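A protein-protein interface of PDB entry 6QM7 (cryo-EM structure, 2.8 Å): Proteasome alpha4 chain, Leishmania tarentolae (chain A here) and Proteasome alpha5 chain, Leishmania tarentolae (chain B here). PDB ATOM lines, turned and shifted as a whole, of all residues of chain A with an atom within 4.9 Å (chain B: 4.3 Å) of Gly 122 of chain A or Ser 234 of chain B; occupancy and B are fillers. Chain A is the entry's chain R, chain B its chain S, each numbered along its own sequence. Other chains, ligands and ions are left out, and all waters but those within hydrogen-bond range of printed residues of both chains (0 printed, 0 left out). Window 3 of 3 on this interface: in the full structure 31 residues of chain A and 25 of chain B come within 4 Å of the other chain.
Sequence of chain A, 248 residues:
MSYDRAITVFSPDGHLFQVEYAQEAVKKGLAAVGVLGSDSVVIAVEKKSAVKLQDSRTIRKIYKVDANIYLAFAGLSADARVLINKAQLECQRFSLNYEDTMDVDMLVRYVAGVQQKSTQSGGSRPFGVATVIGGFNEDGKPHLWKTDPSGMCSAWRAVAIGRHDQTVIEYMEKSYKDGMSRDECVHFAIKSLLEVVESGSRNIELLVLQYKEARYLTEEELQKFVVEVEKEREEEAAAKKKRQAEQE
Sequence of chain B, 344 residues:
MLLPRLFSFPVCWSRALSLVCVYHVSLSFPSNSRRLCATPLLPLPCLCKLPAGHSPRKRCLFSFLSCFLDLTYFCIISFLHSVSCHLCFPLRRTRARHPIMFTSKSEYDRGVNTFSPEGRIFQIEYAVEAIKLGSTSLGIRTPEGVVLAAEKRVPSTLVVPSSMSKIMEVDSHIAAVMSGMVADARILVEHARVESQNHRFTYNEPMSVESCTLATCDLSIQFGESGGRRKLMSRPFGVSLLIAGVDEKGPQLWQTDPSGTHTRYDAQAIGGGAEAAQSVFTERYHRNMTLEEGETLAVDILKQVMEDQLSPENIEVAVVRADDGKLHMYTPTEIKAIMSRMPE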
ATOM      1  N   TYR A   3     -21.957  25.015 -20.878  1.00  0.00           N
ATOM      2  CA  TYR A   3     -21.402  24.202 -19.769  1.00  0.00           C
ATOM      3  C   TYR A   3     -22.454  23.189 -19.325  1.00  0.00           C
ATOM      4  O   TYR A   3     -23.430  23.601 -18.677  1.00  0.00           O
ATOM      5  CB  TYR A   3     -20.987  25.115 -18.617  1.00  0.00           C
ATOM      6  CG  TYR A   3     -20.520  24.427 -17.360  1.00  0.00           C
ATOM      7  CD1 TYR A   3     -19.225  23.961 -17.233  1.00  0.00           C
ATOM      8  CD2 TYR A   3     -21.358  24.303 -16.266  1.00  0.00           C
ATOM      9  CE1 TYR A   3     -18.785  23.362 -16.060  1.00  0.00           C
ATOM     10  CE2 TYR A   3     -20.934  23.710 -15.086  1.00  0.00           C
ATOM     11  CZ  TYR A   3     -19.637  23.241 -14.977  1.00  0.00           C
ATOM     12  OH  TYR A   3     -19.224  22.654 -13.818  1.00  0.00           O
ATOM     13  N   ASP A   4     -22.258  21.921 -19.693  1.00  0.00           N
ATOM     14  CA  ASP A   4     -23.150  20.784 -19.351  1.00  0.00           C
ATOM     15  C   ASP A   4     -22.318  19.699 -18.671  1.00  0.00           C
ATOM     16  O   ASP A   4     -22.560  18.526 -18.962  1.00  0.00           O
ATOM     17  CB  ASP A   4     -23.932  20.277 -20.576  1.00  0.00           C
ATOM     18  CG  ASP A   4     -23.118  19.816 -21.789  1.00  0.00           C
ATOM     19  OD1 ASP A   4     -21.942  19.413 -21.618  1.00  0.00           O
ATOM     20  OD2 ASP A   4     -23.680  19.855 -22.912  1.00  0.00           O
ATOM     21  N   ARG A   5     -21.397  20.080 -17.782  1.00  0.00           N
ATOM     22  CA  ARG A   5     -20.722  19.119 -16.872  1.00  0.00           C
ATOM     23  C   ARG A   5     -21.781  18.514 -15.944  1.00  0.00           C
ATOM     24  O   ARG A   5     -22.733  19.231 -15.594  1.00  0.00           O
ATOM     25  CB  ARG A   5     -19.615  19.794 -16.055  1.00  0.00           C
ATOM     26  CG  ARG A   5     -18.647  18.828 -15.377  1.00  0.00           C
ATOM     27  CD  ARG A   5     -18.497  19.098 -13.888  1.00  0.00           C
ATOM     28  NE  ARG A   5     -17.117  19.062 -13.397  1.00  0.00           N
ATOM     29  CZ  ARG A   5     -16.445  17.976 -13.005  1.00  0.00           C
ATOM     30  NH1 ARG A   5     -16.990  16.770 -13.057  1.00  0.00           N
ATOM     31  NH2 ARG A   5     -15.203  18.102 -12.568  1.00  0.00           N
ATOM     32  N   ALA A   6     -21.632  17.240 -15.588  1.00  0.00           N
ATOM     33  CA  ALA A   6     -22.539  16.512 -14.668  1.00  0.00           C
ATOM     34  C   ALA A   6     -22.248  16.938 -13.229  1.00  0.00           C
ATOM     35  O   ALA A   6     -21.141  16.639 -12.740  1.00  0.00           O
ATOM     36  CB  ALA A   6     -22.369  15.020 -14.822  1.00  0.00           C
ATOM     37  N   ILE A   7     -23.215  17.588 -12.580  1.00  0.00           N
ATOM     38  CA  ILE A   7     -23.081  18.141 -11.199  1.00  0.00           C
ATOM     39  C   ILE A   7     -23.761  17.183 -10.216  1.00  0.00           C
ATOM     40  O   ILE A   7     -23.175  16.893  -9.163  1.00  0.00           O
ATOM     41  CB  ILE A   7     -23.631  19.584 -11.151  1.00  0.00           C
ATOM     42  CG1 ILE A   7     -22.602  20.586 -11.686  1.00  0.00           C
ATOM     43  CG2 ILE A   7     -24.102  19.978  -9.762  1.00  0.00           C
ATOM     44  CD1 ILE A   7     -23.209  21.726 -12.471  1.00  0.00           C
ATOM     45  N   THR A   8     -24.969  16.733 -10.529  1.00  0.00           N
ATOM     46  CA  THR A   8     -25.726  15.786  -9.679  1.00  0.00           C
ATOM     47  C   THR A   8     -25.388  14.381 -10.163  1.00  0.00           C
ATOM     48  O   THR A   8     -25.792  14.047 -11.296  1.00  0.00           O
ATOM     49  CB  THR A   8     -27.230  16.069  -9.703  1.00  0.00           C
ATOM     50  OG1 THR A   8     -27.488  17.472  -9.583  1.00  0.00           O
ATOM     51  CG2 THR A   8     -27.942  15.331  -8.591  1.00  0.00           C
ATOM     52  N   THR A 119     -32.076  18.072 -10.810  1.00  0.00           N
ATOM     53  CA  THR A 119     -31.234  16.988 -10.235  1.00  0.00           C
ATOM     54  C   THR A 119     -30.653  16.090 -11.328  1.00  0.00           C
ATOM     55  O   THR A 119     -29.977  15.127 -10.946  1.00  0.00           O
ATOM     56  CB  THR A 119     -31.985  16.136  -9.204  1.00  0.00           C
ATOM     57  OG1 THR A 119     -32.754  15.111  -9.838  1.00  0.00           O
ATOM     58  CG2 THR A 119     -32.881  16.965  -8.312  1.00  0.00           C
ATOM     59  N   GLN A 120     -30.947  16.338 -12.607  1.00  0.00           N
ATOM     60  CA  GLN A 120     -30.495  15.471 -13.732  1.00  0.00           C
ATOM     61  C   GLN A 120     -30.004  16.299 -14.925  1.00  0.00           C
ATOM     62  O   GLN A 120     -29.431  15.706 -15.844  1.00  0.00           O
ATOM     63  CB  GLN A 120     -31.618  14.524 -14.160  1.00  0.00           C
ATOM     64  CG  GLN A 120     -31.138  13.113 -14.502  1.00  0.00           C
ATOM     65  CD  GLN A 120     -32.274  12.144 -14.740  1.00  0.00           C
ATOM     66  OE1 GLN A 120     -33.441  12.529 -14.818  1.00  0.00           O
ATOM     67  NE2 GLN A 120     -31.939  10.870 -14.857  1.00  0.00           N
ATOM     68  N   SER A 121     -30.217  17.610 -14.924  1.00  0.00           N
ATOM     69  CA  SER A 121     -29.644  18.549 -15.915  1.00  0.00           C
ATOM     70  C   SER A 121     -28.135  18.632 -15.680  1.00  0.00           C
ATOM     71  O   SER A 121     -27.719  18.932 -14.539  1.00  0.00           O
ATOM     72  CB  SER A 121     -30.295  19.915 -15.820  1.00  0.00           C
ATOM     73  OG  SER A 121     -29.935  20.732 -16.928  1.00  0.00           O
ATOM     74  N   GLY A 122     -27.352  18.329 -16.709  1.00  0.00           N
ATOM     75  CA  GLY A 122     -25.930  18.687 -16.746  1.00  0.00           C
ATOM     76  C   GLY A 122     -25.801  20.192 -16.803  1.00  0.00           C
ATOM     77  O   GLY A 122     -26.495  20.809 -17.645  1.00  0.00           O
ATOM     78  N   GLY A 123     -24.981  20.762 -15.918  1.00  0.00           N
ATOM     79  CA  GLY A 123     -24.654  22.200 -15.896  1.00  0.00           C
ATOM     80  C   GLY A 123     -25.283  22.918 -14.720  1.00  0.00           C
ATOM     81  O   GLY A 123     -24.834  24.043 -14.413  1.00  0.00           O
ATOM     82  N   SER A 124     -26.271  22.306 -14.074  1.00  0.00           N
ATOM     83  CA  SER A 124     -27.060  22.931 -12.986  1.00  0.00           C
ATOM     84  C   SER A 124     -26.912  22.118 -11.702  1.00  0.00           C
ATOM     85  O   SER A 124     -26.873  20.863 -11.771  1.00  0.00           O
ATOM     86  CB  SER A 124     -28.510  23.068 -13.380  1.00  0.00           C
ATOM     87  OG  SER A 124     -28.641  23.131 -14.799  1.00  0.00           O
ATOM     88  N   VAL B 112     -18.559  10.521 -15.406  1.00  0.00           N
ATOM     89  CA  VAL B 112     -19.855   9.779 -15.408  1.00  0.00           C
ATOM     90  C   VAL B 112     -19.736   8.507 -16.269  1.00  0.00           C
ATOM     91  O   VAL B 112     -20.330   7.473 -15.882  1.00  0.00           O
ATOM     92  CB  VAL B 112     -20.980  10.724 -15.886  1.00  0.00           C
ATOM     93  CG1 VAL B 112     -22.146   9.994 -16.534  1.00  0.00           C
ATOM     94  CG2 VAL B 112     -21.463  11.613 -14.748  1.00  0.00           C
ATOM     95  N   GLY B 224     -24.973  11.430 -20.033  1.00  0.00           N
ATOM     96  CA  GLY B 224     -23.571  11.861 -20.226  1.00  0.00           C
ATOM     97  C   GLY B 224     -23.189  12.983 -19.272  1.00  0.00           C
ATOM     98  O   GLY B 224     -22.379  13.835 -19.686  1.00  0.00           O
ATOM     99  N   LEU B 232     -26.957  14.246 -22.388  1.00  0.00           N
ATOM    100  CA  LEU B 232     -28.241  14.997 -22.274  1.00  0.00           C
ATOM    101  C   LEU B 232     -28.649  15.092 -20.792  1.00  0.00           C
ATOM    102  O   LEU B 232     -28.853  16.226 -20.302  1.00  0.00           O
ATOM    103  CB  LEU B 232     -29.330  14.300 -23.105  1.00  0.00           C
ATOM    104  CG  LEU B 232     -29.184  14.381 -24.629  1.00  0.00           C
ATOM    105  CD1 LEU B 232     -28.118  13.421 -25.150  1.00  0.00           C
ATOM    106  CD2 LEU B 232     -30.522  14.118 -25.318  1.00  0.00           C
ATOM    107  N   MET B 233     -28.762  13.939 -20.119  1.00  0.00           N
ATOM    108  CA  MET B 233     -28.995  13.800 -18.653  1.00  0.00           C
ATOM    109  C   MET B 233     -27.655  13.528 -17.951  1.00  0.00           C
ATOM    110  O   MET B 233     -26.924  12.637 -18.401  1.00  0.00           O
ATOM    111  CB  MET B 233     -29.940  12.633 -18.361  1.00  0.00           C
ATOM    112  CG  MET B 233     -31.417  12.961 -18.535  1.00  0.00           C
ATOM    113  SD  MET B 233     -32.396  11.541 -19.119  1.00  0.00           S
ATOM    114  CE  MET B 233     -31.438  10.139 -18.522  1.00  0.00           C
ATOM    115  N   SER B 234     -27.358  14.266 -16.883  1.00  0.00           N
ATOM    116  CA  SER B 234     -26.081  14.183 -16.130  1.00  0.00           C
ATOM    117  C   SER B 234     -25.806  12.734 -15.705  1.00  0.00           C
ATOM    118  O   SER B 234     -24.675  12.272 -15.909  1.00  0.00           O
ATOM    119  CB  SER B 234     -26.065  15.138 -14.928  1.00  0.00           C
ATOM    120  OG  SER B 234     -27.117  14.895 -13.999  1.00  0.00           O
ATOM    121  N   ARG B 235     -26.817  12.045 -15.178  1.00  0.00           N
ATOM    122  CA  ARG B 235     -26.669  10.767 -14.438  1.00  0.00           C
ATOM    123  C   ARG B 235     -27.745   9.799 -14.896  1.00  0.00           C
ATOM    124  O   ARG B 235     -28.738  10.229 -15.471  1.00  0.00           O
ATOM    125  CB  ARG B 235     -26.880  10.991 -12.937  1.00  0.00           C
ATOM    126  CG  ARG B 235     -28.194  11.689 -12.622  1.00  0.00           C
ATOM    127  CD  ARG B 235     -28.471  11.814 -11.161  1.00  0.00           C
ATOM    128  NE  ARG B 235     -29.742  12.496 -10.976  1.00  0.00           N
ATOM    129  CZ  ARG B 235     -30.929  11.906 -10.932  1.00  0.00           C
ATOM    130  NH1 ARG B 235     -31.044  10.590 -11.050  1.00  0.00           N
ATOM    131  NH2 ARG B 235     -32.010  12.645 -10.760  1.00  0.00           N
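The backbone NH (N) of Ser 234 of chain B is in hydrogen-bond range of the backbone carbonyl oxygen (O) of Gln 120 of chain A, at 2.7 Å.
The side-chain amide nitrogen (NE2) of Gln 120 of chain A lies within hydrogen-bond range of the backbone carbonyl oxygen (O) of Arg 235 of chain B.
The backbone carbonyl oxygen (O) of Thr 8 of chain A lies within hydrogen-bond range of the side-chain hydroxyl (OG) of Ser 234 of chain B (3.1 Å).
The backbone carbonyl oxygen (O) of Thr 119 of chain A sits at hydrogen-bond distance from the guanidinium group (NE) of Arg 235 of chain B (2.6 Å).
N of Gly 224 of chain B sits at hydrogen-bond distance from O of Met 233 of chain B (2.8 Å).
Val 112 of chain B touches Ala 6 of chain A (CG2 to CB, 3.5 Å).
Ser 234 of chain B touches Ala 6 of chain A (CB to CB, 3.7 Å).
Arg 235 of chain B touches Thr 8 of chain A (CD to O, 3.5 Å).
O of Gln 120 of chain A touches CA of Met 233 of chain B (3.4 Å).
Gly 122 of chain A touches Ser 234 of chain B (N to CB, 3.9 Å).
Of the printed residues of chain B, Gly 122 of chain A touches Ser 234 (3.9 Å).
Ser 234 of chain B touches just these residues of chain A: Ala 6, Thr 8, Gln 120 and Gly 122.
Printed residues of chain A within 4 Å of Val 112 of chain B: Ala 6 (3.5 Å).
Of the printed residues of chain B, Gln 120 of chain A touches Met 233, Ser 234 and Arg 235.
Leu 232 of chain B touches none of the printed residues of chain A.
Tyr 3 of chain A touches none of the printed residues of chain B.
Hydrophobic or aromatic side chains of chain B within 4 Å of the printed part of chain A: Val 112 and Met 233.
Among the printed residues, no Asp or Glu carboxylate lies within 4 Å of a Lys or Arg side-chain nitrogen of the other chain.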
